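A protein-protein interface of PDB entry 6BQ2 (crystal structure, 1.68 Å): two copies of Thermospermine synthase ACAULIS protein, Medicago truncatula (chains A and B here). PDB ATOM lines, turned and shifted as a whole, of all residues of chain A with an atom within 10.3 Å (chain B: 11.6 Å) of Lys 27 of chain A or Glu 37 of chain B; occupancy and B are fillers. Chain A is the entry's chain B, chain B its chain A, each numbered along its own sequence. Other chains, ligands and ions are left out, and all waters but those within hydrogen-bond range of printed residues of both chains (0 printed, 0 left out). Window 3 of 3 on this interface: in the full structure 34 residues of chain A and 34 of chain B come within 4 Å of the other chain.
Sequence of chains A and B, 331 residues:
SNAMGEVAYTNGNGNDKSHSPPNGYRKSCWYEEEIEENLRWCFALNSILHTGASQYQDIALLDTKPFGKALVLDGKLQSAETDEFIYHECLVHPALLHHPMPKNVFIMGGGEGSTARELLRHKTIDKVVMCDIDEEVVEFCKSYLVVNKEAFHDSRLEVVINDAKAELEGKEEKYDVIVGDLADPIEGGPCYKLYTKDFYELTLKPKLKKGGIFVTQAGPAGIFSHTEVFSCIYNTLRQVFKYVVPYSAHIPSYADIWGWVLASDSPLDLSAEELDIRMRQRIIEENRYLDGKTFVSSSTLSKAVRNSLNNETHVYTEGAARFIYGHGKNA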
ATOM      1  N   LYS A  27     -26.690  21.785 -12.986  1.00  0.00           N
ATOM      2  CA  LYS A  27     -26.228  22.077 -11.599  1.00  0.00           C
ATOM      3  C   LYS A  27     -26.806  21.015 -10.663  1.00  0.00           C
ATOM      4  O   LYS A  27     -28.014  21.022 -10.389  1.00  0.00           O
ATOM      5  CB  LYS A  27     -26.675  23.483 -11.147  1.00  0.00           C
ATOM      6  CG  LYS A  27     -26.385  24.622 -12.123  1.00  0.00           C
ATOM      7  CD  LYS A  27     -24.906  24.709 -12.514  1.00  0.00           C
ATOM      8  CE  LYS A  27     -24.569  25.856 -13.482  1.00  0.00           C
ATOM      9  NZ  LYS A  27     -25.651  26.255 -14.438  1.00  0.00           N
ATOM     10  N   SER A  28     -25.943  20.114 -10.179  1.00  0.00           N
ATOM     11  CA  SER A  28     -26.366  19.013  -9.335  1.00  0.00           C
ATOM     12  C   SER A  28     -26.091  19.205  -7.852  1.00  0.00           C
ATOM     13  O   SER A  28     -26.774  18.556  -7.066  1.00  0.00           O
ATOM     14  CB  SER A  28     -25.750  17.690  -9.805  1.00  0.00           C
ATOM     15  OG  SER A  28     -24.385  17.559  -9.430  1.00  0.00           O
ATOM     16  N   CYS A  29     -25.118  20.052  -7.461  1.00  0.00           N
ATOM     17  CA  CYS A  29     -24.757  20.173  -6.052  1.00  0.00           C
ATOM     18  C   CYS A  29     -25.223  21.516  -5.488  1.00  0.00           C
ATOM     19  O   CYS A  29     -25.001  22.542  -6.109  1.00  0.00           O
ATOM     20  CB  CYS A  29     -23.244  20.005  -5.827  1.00  0.00           C
ATOM     21  SG  CYS A  29     -22.684  18.322  -6.218  1.00  0.00           S
ATOM     22  N   TRP A  30     -25.835  21.467  -4.307  1.00  0.00           N
ATOM     23  CA  TRP A  30     -26.515  22.606  -3.708  1.00  0.00           C
ATOM     24  C   TRP A  30     -26.217  22.736  -2.222  1.00  0.00           C
ATOM     25  O   TRP A  30     -26.170  21.743  -1.524  1.00  0.00           O
ATOM     26  CB  TRP A  30     -28.052  22.481  -3.887  1.00  0.00           C
ATOM     27  CG  TRP A  30     -28.494  22.543  -5.319  1.00  0.00           C
ATOM     28  CD1 TRP A  30     -28.663  21.491  -6.167  1.00  0.00           C
ATOM     29  CD2 TRP A  30     -28.789  23.722  -6.073  1.00  0.00           C
ATOM     30  NE1 TRP A  30     -29.036  21.943  -7.416  1.00  0.00           N
ATOM     31  CE2 TRP A  30     -29.126  23.309  -7.385  1.00  0.00           C
ATOM     32  CE3 TRP A  30     -28.820  25.094  -5.765  1.00  0.00           C
ATOM     33  CZ2 TRP A  30     -29.480  24.218  -8.394  1.00  0.00           C
ATOM     34  CZ3 TRP A  30     -29.165  26.004  -6.771  1.00  0.00           C
ATOM     35  CH2 TRP A  30     -29.494  25.563  -8.069  1.00  0.00           C
ATOM     36  N   TYR A  31     -26.047  23.968  -1.770  1.00  0.00           N
ATOM     37  CA  TYR A  31     -26.097  24.322  -0.369  1.00  0.00           C
ATOM     38  C   TYR A  31     -27.507  24.802  -0.081  1.00  0.00           C
ATOM     39  O   TYR A  31     -27.992  25.663  -0.776  1.00  0.00           O
ATOM     40  CB  TYR A  31     -25.146  25.467  -0.041  1.00  0.00           C
ATOM     41  CG  TYR A  31     -25.390  26.049   1.309  1.00  0.00           C
ATOM     42  CD1 TYR A  31     -25.073  25.346   2.454  1.00  0.00           C
ATOM     43  CD2 TYR A  31     -25.999  27.313   1.460  1.00  0.00           C
ATOM     44  CE1 TYR A  31     -25.331  25.862   3.707  1.00  0.00           C
ATOM     45  CE2 TYR A  31     -26.224  27.833   2.705  1.00  0.00           C
ATOM     46  CZ  TYR A  31     -25.899  27.090   3.829  1.00  0.00           C
ATOM     47  OH  TYR A  31     -26.144  27.634   5.076  1.00  0.00           O
ATOM     48  N   CYS A  42     -31.523  28.077  -1.842  1.00  0.00           N
ATOM     49  CA  CYS A  42     -30.539  27.088  -2.270  1.00  0.00           C
ATOM     50  C   CYS A  42     -29.548  27.760  -3.186  1.00  0.00           C
ATOM     51  O   CYS A  42     -29.956  28.501  -4.072  1.00  0.00           O
ATOM     52  CB  CYS A  42     -31.199  25.896  -2.951  1.00  0.00           C
ATOM     53  SG  CYS A  42     -32.637  25.309  -1.991  1.00  0.00           S
ATOM     54  N   PHE A  43     -28.260  27.535  -2.928  1.00  0.00           N
ATOM     55  CA  PHE A  43     -27.150  28.119  -3.717  1.00  0.00           C
ATOM     56  C   PHE A  43     -26.410  26.960  -4.395  1.00  0.00           C
ATOM     57  O   PHE A  43     -26.050  25.986  -3.744  1.00  0.00           O
ATOM     58  CB  PHE A  43     -26.073  28.803  -2.859  1.00  0.00           C
ATOM     59  CG  PHE A  43     -26.563  29.707  -1.827  1.00  0.00           C
ATOM     60  CD1 PHE A  43     -27.715  30.429  -1.990  1.00  0.00           C
ATOM     61  CD2 PHE A  43     -25.777  29.924  -0.694  1.00  0.00           C
ATOM     62  CE1 PHE A  43     -28.126  31.310  -1.021  1.00  0.00           C
ATOM     63  CE2 PHE A  43     -26.180  30.790   0.270  1.00  0.00           C
ATOM     64  CZ  PHE A  43     -27.349  31.507   0.117  1.00  0.00           C
ATOM     65  N   ALA A  44     -26.145  27.079  -5.692  1.00  0.00           N
ATOM     66  CA  ALA A  44     -25.331  26.067  -6.367  1.00  0.00           C
ATOM     67  C   ALA A  44     -23.895  26.090  -5.779  1.00  0.00           C
ATOM     68  O   ALA A  44     -23.359  27.165  -5.474  1.00  0.00           O
ATOM     69  CB  ALA A  44     -25.317  26.313  -7.857  1.00  0.00           C
ATOM     70  N   LEU A  45     -23.314  24.898  -5.606  1.00  0.00           N
ATOM     71  CA  LEU A  45     -22.023  24.673  -4.955  1.00  0.00           C
ATOM     72  C   LEU A  45     -20.966  24.280  -5.999  1.00  0.00           C
ATOM     73  O   LEU A  45     -21.230  23.370  -6.821  1.00  0.00           O
ATOM     74  CB  LEU A  45     -22.107  23.513  -3.980  1.00  0.00           C
ATOM     75  CG  LEU A  45     -22.558  23.638  -2.552  1.00  0.00           C
ATOM     76  CD1 LEU A  45     -22.413  22.270  -1.886  1.00  0.00           C
ATOM     77  CD2 LEU A  45     -21.750  24.667  -1.801  1.00  0.00           C
ATOM     78  N   ASN A  46     -19.821  24.969  -5.961  1.00  0.00           N
ATOM     79  CA  ASN A  46     -18.590  24.535  -6.664  1.00  0.00           C
ATOM     80  C   ASN A  46     -17.827  23.502  -5.835  1.00  0.00           C
ATOM     81  O   ASN A  46     -17.356  22.509  -6.387  1.00  0.00           O
ATOM     82  CB  ASN A  46     -17.653  25.709  -6.977  1.00  0.00           C
ATOM     83  CG  ASN A  46     -18.184  26.642  -8.047  1.00  0.00           C
ATOM     84  OD1 ASN A  46     -18.721  26.212  -9.047  1.00  0.00           O
ATOM     85  ND2 ASN A  46     -17.998  27.926  -7.847  1.00  0.00           N
ATOM     86  N   THR A  64     -19.380  28.725  -3.325  1.00  0.00           N
ATOM     87  CA  THR A  64     -20.708  28.797  -3.973  1.00  0.00           C
ATOM     88  C   THR A  64     -20.653  29.584  -5.240  1.00  0.00           C
ATOM     89  O   THR A  64     -19.872  30.513  -5.369  1.00  0.00           O
ATOM     90  CB  THR A  64     -21.776  29.442  -3.044  1.00  0.00           C
ATOM     91  OG1 THR A  64     -21.598  30.860  -2.992  1.00  0.00           O
ATOM     92  CG2 THR A  64     -21.649  28.919  -1.618  1.00  0.00           C
ATOM     93  N   LYS A  65     -21.569  29.278  -6.155  1.00  0.00           N
ATOM     94  CA  LYS A  65     -21.629  29.974  -7.426  1.00  0.00           C
ATOM     95  C   LYS A  65     -22.163  31.369  -7.279  1.00  0.00           C
ATOM     96  O   LYS A  65     -21.502  32.305  -7.749  1.00  0.00           O
ATOM     97  CB  LYS A  65     -22.406  29.185  -8.455  1.00  0.00           C
ATOM     98  CG  LYS A  65     -21.631  27.953  -8.927  1.00  0.00           C
ATOM     99  CD  LYS A  65     -22.396  27.140  -9.957  1.00  0.00           C
ATOM    100  CE  LYS A  65     -21.814  25.747 -10.089  1.00  0.00           C
ATOM    101  NZ  LYS A  65     -20.562  25.849 -10.876  1.00  0.00           N
ATOM    102  N   PRO A  66     -23.336  31.548  -6.616  1.00  0.00           N
ATOM    103  CA  PRO A  66     -23.850  32.931  -6.569  1.00  0.00           C
ATOM    104  C   PRO A  66     -23.027  33.883  -5.677  1.00  0.00           C
ATOM    105  O   PRO A  66     -22.839  35.059  -6.017  1.00  0.00           O
ATOM    106  CB  PRO A  66     -25.284  32.762  -6.063  1.00  0.00           C
ATOM    107  CG  PRO A  66     -25.294  31.450  -5.390  1.00  0.00           C
ATOM    108  CD  PRO A  66     -24.292  30.569  -6.078  1.00  0.00           C
ATOM    109  N   PHE A  67     -22.502  33.402  -4.577  1.00  0.00           N
ATOM    110  CA  PHE A  67     -21.955  34.289  -3.562  1.00  0.00           C
ATOM    111  C   PHE A  67     -20.478  34.108  -3.266  1.00  0.00           C
ATOM    112  O   PHE A  67     -19.965  34.704  -2.324  1.00  0.00           O
ATOM    113  CB  PHE A  67     -22.796  34.131  -2.286  1.00  0.00           C
ATOM    114  CG  PHE A  67     -24.254  34.474  -2.489  1.00  0.00           C
ATOM    115  CD1 PHE A  67     -24.608  35.710  -3.010  1.00  0.00           C
ATOM    116  CD2 PHE A  67     -25.259  33.546  -2.224  1.00  0.00           C
ATOM    117  CE1 PHE A  67     -25.935  36.053  -3.234  1.00  0.00           C
ATOM    118  CE2 PHE A  67     -26.596  33.887  -2.441  1.00  0.00           C
ATOM    119  CZ  PHE A  67     -26.937  35.130  -2.945  1.00  0.00           C
ATOM    120  N   GLU B  32     -41.253  25.467  -5.806  1.00  0.00           N
ATOM    121  CA  GLU B  32     -39.866  25.765  -6.082  1.00  0.00           C
ATOM    122  C   GLU B  32     -39.773  26.654  -7.307  1.00  0.00           C
ATOM    123  O   GLU B  32     -40.486  26.442  -8.284  1.00  0.00           O
ATOM    124  CB  GLU B  32     -39.185  24.440  -6.338  1.00  0.00           C
ATOM    125  CG  GLU B  32     -37.714  24.498  -6.580  1.00  0.00           C
ATOM    126  CD  GLU B  32     -37.179  23.086  -6.718  1.00  0.00           C
ATOM    127  OE1 GLU B  32     -37.127  22.385  -5.675  1.00  0.00           O
ATOM    128  OE2 GLU B  32     -36.898  22.680  -7.868  1.00  0.00           O
ATOM    129  N   GLU B  33     -38.948  27.683  -7.230  1.00  0.00           N
ATOM    130  CA  GLU B  33     -38.673  28.544  -8.353  1.00  0.00           C
ATOM    131  C   GLU B  33     -37.192  28.869  -8.423  1.00  0.00           C
ATOM    132  O   GLU B  33     -36.544  29.152  -7.420  1.00  0.00           O
ATOM    133  CB  GLU B  33     -39.514  29.825  -8.248  1.00  0.00           C
ATOM    134  CG  GLU B  33     -39.236  30.804  -9.381  1.00  0.00           C
ATOM    135  CD  GLU B  33     -40.267  31.904  -9.515  1.00  0.00           C
ATOM    136  OE1 GLU B  33     -41.349  31.784  -8.905  1.00  0.00           O
ATOM    137  OE2 GLU B  33     -40.004  32.875 -10.273  1.00  0.00           O
ATOM    138  N   GLU B  34     -36.674  28.859  -9.647  1.00  0.00           N
ATOM    139  CA  GLU B  34     -35.308  29.242  -9.919  1.00  0.00           C
ATOM    140  C   GLU B  34     -35.331  30.757 -10.097  1.00  0.00           C
ATOM    141  O   GLU B  34     -35.930  31.254 -11.029  1.00  0.00           O
ATOM    142  CB  GLU B  34     -34.805  28.558 -11.204  1.00  0.00           C
ATOM    143  CG  GLU B  34     -33.297  28.343 -11.255  1.00  0.00           C
ATOM    144  CD  GLU B  34     -32.696  28.381 -12.682  1.00  0.00           C
ATOM    145  OE1 GLU B  34     -31.720  27.618 -12.912  1.00  0.00           O
ATOM    146  OE2 GLU B  34     -33.162  29.162 -13.568  1.00  0.00           O
ATOM    147  N   ILE B  35     -34.726  31.477  -9.173  1.00  0.00           N
ATOM    148  CA  ILE B  35     -34.609  32.927  -9.286  1.00  0.00           C
ATOM    149  C   ILE B  35     -33.587  33.314 -10.337  1.00  0.00           C
ATOM    150  O   ILE B  35     -33.808  34.281 -11.077  1.00  0.00           O
ATOM    151  CB  ILE B  35     -34.173  33.559  -7.938  1.00  0.00           C
ATOM    152  CG1 ILE B  35     -35.232  33.397  -6.840  1.00  0.00           C
ATOM    153  CG2 ILE B  35     -33.741  35.023  -8.103  1.00  0.00           C
ATOM    154  CD1 ILE B  35     -34.413  33.311  -5.560  1.00  0.00           C
ATOM    155  N   GLU B  36     -32.468  32.607 -10.343  1.00  0.00           N
ATOM    156  CA  GLU B  36     -31.391  32.757 -11.330  1.00  0.00           C
ATOM    157  C   GLU B  36     -30.799  31.383 -11.543  1.00  0.00           C
ATOM    158  O   GLU B  36     -31.079  30.471 -10.777  1.00  0.00           O
ATOM    159  CB  GLU B  36     -30.268  33.659 -10.799  1.00  0.00           C
ATOM    160  CG  GLU B  36     -30.625  35.125 -10.600  1.00  0.00           C
ATOM    161  CD  GLU B  36     -29.534  35.891  -9.854  1.00  0.00           C
ATOM    162  OE1 GLU B  36     -28.330  35.502  -9.941  1.00  0.00           O
ATOM    163  OE2 GLU B  36     -29.875  36.891  -9.178  1.00  0.00           O
ATOM    164  N   GLU B  37     -29.910  31.231 -12.522  1.00  0.00           N
ATOM    165  CA  GLU B  37     -29.358  29.894 -12.784  1.00  0.00           C
ATOM    166  C   GLU B  37     -28.725  29.192 -11.579  1.00  0.00           C
ATOM    167  O   GLU B  37     -28.741  27.960 -11.518  1.00  0.00           O
ATOM    168  CB  GLU B  37     -28.406  29.882 -13.978  1.00  0.00           C
ATOM    169  CG  GLU B  37     -27.129  30.680 -13.844  1.00  0.00           C
ATOM    170  CD  GLU B  37     -26.197  30.382 -15.008  1.00  0.00           C
ATOM    171  OE1 GLU B  37     -26.657  30.509 -16.157  1.00  0.00           O
ATOM    172  OE2 GLU B  37     -25.030  29.996 -14.773  1.00  0.00           O
ATOM    173  N   ASN B  38     -28.184  29.942 -10.623  1.00  0.00           N
ATOM    174  CA  ASN B  38     -27.487  29.303  -9.509  1.00  0.00           C
ATOM    175  C   ASN B  38     -28.155  29.482  -8.127  1.00  0.00           C
ATOM    176  O   ASN B  38     -27.545  29.216  -7.088  1.00  0.00           O
ATOM    177  CB  ASN B  38     -26.052  29.809  -9.489  1.00  0.00           C
ATOM    178  CG  ASN B  38     -25.238  29.317 -10.669  1.00  0.00           C
ATOM    179  OD1 ASN B  38     -24.405  30.047 -11.195  1.00  0.00           O
ATOM    180  ND2 ASN B  38     -25.466  28.073 -11.087  1.00  0.00           N
ATOM    181  N   LEU B  39     -29.414  29.907  -8.145  1.00  0.00           N
ATOM    182  CA  LEU B  39     -30.110  30.333  -6.946  1.00  0.00           C
ATOM    183  C   LEU B  39     -31.570  29.912  -7.063  1.00  0.00           C
ATOM    184  O   LEU B  39     -32.231  30.277  -8.063  1.00  0.00           O
ATOM    185  CB  LEU B  39     -29.991  31.855  -6.886  1.00  0.00           C
ATOM    186  CG  LEU B  39     -30.290  32.648  -5.631  1.00  0.00           C
ATOM    187  CD1 LEU B  39     -29.554  32.126  -4.401  1.00  0.00           C
ATOM    188  CD2 LEU B  39     -29.902  34.093  -5.951  1.00  0.00           C
ATOM    189  N   ARG B  40     -32.032  29.118  -6.096  1.00  0.00           N
ATOM    190  CA  ARG B  40     -33.440  28.631  -6.045  1.00  0.00           C
ATOM    191  C   ARG B  40     -34.066  28.954  -4.703  1.00  0.00           C
ATOM    192  O   ARG B  40     -33.393  28.939  -3.704  1.00  0.00           O
ATOM    193  CB  ARG B  40     -33.522  27.104  -6.216  1.00  0.00           C
ATOM    194  CG  ARG B  40     -32.960  26.579  -7.510  1.00  0.00           C
ATOM    195  CD  ARG B  40     -33.173  25.063  -7.672  1.00  0.00           C
ATOM    196  NE  ARG B  40     -32.794  24.312  -6.476  1.00  0.00           N
ATOM    197  CZ  ARG B  40     -32.776  22.979  -6.393  1.00  0.00           C
ATOM    198  NH1 ARG B  40     -33.121  22.206  -7.426  1.00  0.00           N
ATOM    199  NH2 ARG B  40     -32.404  22.409  -5.243  1.00  0.00           N
ATOM    200  N   TRP B  41     -35.369  29.235  -4.745  1.00  0.00           N
ATOM    201  CA  TRP B  41     -36.241  29.662  -3.648  1.00  0.00           C
ATOM    202  C   TRP B  41     -37.368  28.620  -3.490  1.00  0.00           C
ATOM    203  O   TRP B  41     -37.942  28.217  -4.496  1.00  0.00           O
ATOM    204  CB  TRP B  41     -36.832  30.988  -4.157  1.00  0.00           C
ATOM    205  CG  TRP B  41     -37.397  32.043  -3.228  1.00  0.00           C
ATOM    206  CD1 TRP B  41     -38.519  32.788  -3.458  1.00  0.00           C
ATOM    207  CD2 TRP B  41     -36.848  32.525  -1.994  1.00  0.00           C
ATOM    208  NE1 TRP B  41     -38.719  33.679  -2.436  1.00  0.00           N
ATOM    209  CE2 TRP B  41     -37.710  33.536  -1.521  1.00  0.00           C
ATOM    210  CE3 TRP B  41     -35.727  32.187  -1.232  1.00  0.00           C
ATOM    211  CZ2 TRP B  41     -37.487  34.211  -0.324  1.00  0.00           C
ATOM    212  CZ3 TRP B  41     -35.506  32.862  -0.041  1.00  0.00           C
ATOM    213  CH2 TRP B  41     -36.382  33.860   0.400  1.00  0.00           C
ATOM    214  N   LYS B  76     -43.626  31.204 -12.544  1.00  0.00           N
ATOM    215  CA  LYS B  76     -42.943  32.360 -11.998  1.00  0.00           C
ATOM    216  C   LYS B  76     -43.967  33.032 -11.119  1.00  0.00           C
ATOM    217  O   LYS B  76     -45.045  33.381 -11.593  1.00  0.00           O
ATOM    218  CB  LYS B  76     -42.541  33.379 -13.091  1.00  0.00           C
ATOM    219  CG  LYS B  76     -41.501  32.912 -14.100  1.00  0.00           C
ATOM    220  CD  LYS B  76     -40.167  32.672 -13.418  1.00  0.00           C
ATOM    221  CE  LYS B  76     -39.097  32.163 -14.379  1.00  0.00           C
ATOM    222  NZ  LYS B  76     -37.961  31.545 -13.627  1.00  0.00           N
ATOM    223  N   PRO B 220     -35.210  43.850 -10.919  1.00  0.00           N
ATOM    224  CA  PRO B 220     -34.406  43.787  -9.668  1.00  0.00           C
ATOM    225  C   PRO B 220     -33.498  44.999  -9.530  1.00  0.00           C
ATOM    226  O   PRO B 220     -32.980  45.546 -10.527  1.00  0.00           O
ATOM    227  CB  PRO B 220     -33.600  42.514  -9.847  1.00  0.00           C
ATOM    228  CG  PRO B 220     -34.394  41.673 -10.797  1.00  0.00           C
ATOM    229  CD  PRO B 220     -34.970  42.666 -11.753  1.00  0.00           C
ATOM    230  N   SER B 225     -27.775  42.776  -8.685  1.00  0.00           N
ATOM    231  CA  SER B 225     -28.843  42.402  -9.607  1.00  0.00           C
ATOM    232  C   SER B 225     -29.348  43.558 -10.406  1.00  0.00           C
ATOM    233  O   SER B 225     -29.956  43.340 -11.483  1.00  0.00           O
ATOM    234  CB  SER B 225     -30.002  41.738  -8.877  1.00  0.00           C
ATOM    235  OG  SER B 225     -30.614  42.601  -7.946  1.00  0.00           O
ATOM    236  N   GLU B 228     -28.906  44.068 -14.466  1.00  0.00           N
ATOM    237  CA  GLU B 228     -29.535  43.222 -15.460  1.00  0.00           C
ATOM    238  C   GLU B 228     -30.400  44.100 -16.349  1.00  0.00           C
ATOM    239  O   GLU B 228     -30.282  44.049 -17.582  1.00  0.00           O
ATOM    240  CB  GLU B 228     -30.472  42.159 -14.859  1.00  0.00           C
ATOM    241  CG  GLU B 228     -29.929  41.128 -13.876  1.00  0.00           C
ATOM    242  CD  GLU B 228     -31.097  40.413 -13.164  1.00  0.00           C
ATOM    243  OE1 GLU B 228     -32.107  40.051 -13.878  1.00  0.00           O
ATOM    244  OE2 GLU B 228     -31.033  40.241 -11.927  1.00  0.00           O
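Glu 37 of chain B touches just one residue of chain A: Lys 27 (3.8 Å). No residue of chain B comes within 4 Å of Ser 28 of chain A. No residue of chain B comes within 4 Å of Cys 29 of chain A. Of chain B, only Asn 38 (2.9 Å) comes within 4 Å of Ala 44 of chain A. Asn 38 of chain B touches seven residues of chain A. Printed residues of chain A within 4 Å of Leu 39 of chain B: Cys 42 (3.4 Å), Phe 43 (3.5 Å) and Phe 67 (3.96 Å). Printed residues of chain B within 4 Å of Lys 65 of chain A: Asn 38. Tyr 31 of chain A touches none of the printed residues of chain B. Glu 32 of chain B touches none of the printed residues of chain A. The nearest residue of chain A that does not touch Glu 37 of chain B is Trp 30 of chain A (4.3 Å).
N of Ala 44 of chain A lies within hydrogen-bond range of O of Asn 38 of chain B, 2.9 Å away. O of Arg 40 of chain B is in hydrogen-bond range of N of Cys 42 of chain A (2.8 Å). OE2 of Glu 37 of chain B is in salt-bridge range of NZ of Lys 27 of chain A, at 3.8 Å.
Among the printed residues, pairs that only touch across the chains: Lys 27 of chain A with Asn 38 of chain B, Trp 30 of chain A with Asn 38 of chain B, Trp 30 of chain A with Arg 40 of chain B, Cys 42 of chain A with Asn 38 of chain B, Cys 42 of chain A with Leu 39 of chain B, Phe 43 of chain A with Asn 38 of chain B, Phe 43 of chain A with Leu 39 of chain B, Lys 65 of chain A with Asn 38 of chain B, Pro 66 of chain A with Asn 38 of chain B and Phe 67 of chain A with Leu 39 of chain B.
O of Lys 27 of chain A lies within hydrogen-bond range of NE1 of Trp 30 of chain A (3.3 Å). N of Tyr 31 of chain A is in hydrogen-bond range of O of Phe 43 of chain A. N of Lys 65 of chain A lies within hydrogen-bond range of O of Ala 44 of chain A (2.9 Å). The guanidinium group (NH1) of Arg 40 of chain B is in salt-bridge range of the side-chain carboxylate (OE2) of Glu 32 of chain B. The backbone NH of Phe 67 of chain A sits at hydrogen-bond distance from the side-chain hydroxyl of Thr 64 of chain A (3.1 Å). The side-chain amide oxygen (OD1) of Asn 46 of chain A sits at hydrogen-bond distance from the side-chain amino group (NZ) of Lys 65 of chain A (2.6 Å).
Printed residues of chain A that touch a printed residue of chain B: Lys 27, Trp 30, Cys 42, Phe 43, Ala 44, Lys 65, Pro 66 and Phe 67. Hydrophobic or aromatic side chains of chain A that line the printed part of chain B: Trp 30, Phe 43, Ala 44, Pro 66 and Phe 67. Of the 14 printed residues of chain B, 4 touch a printed residue of chain A. Hydrophobic or aromatic side chains of chain B within 4 Å of the printed part of chain A: Leu 39.
No position is printed for both chains.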
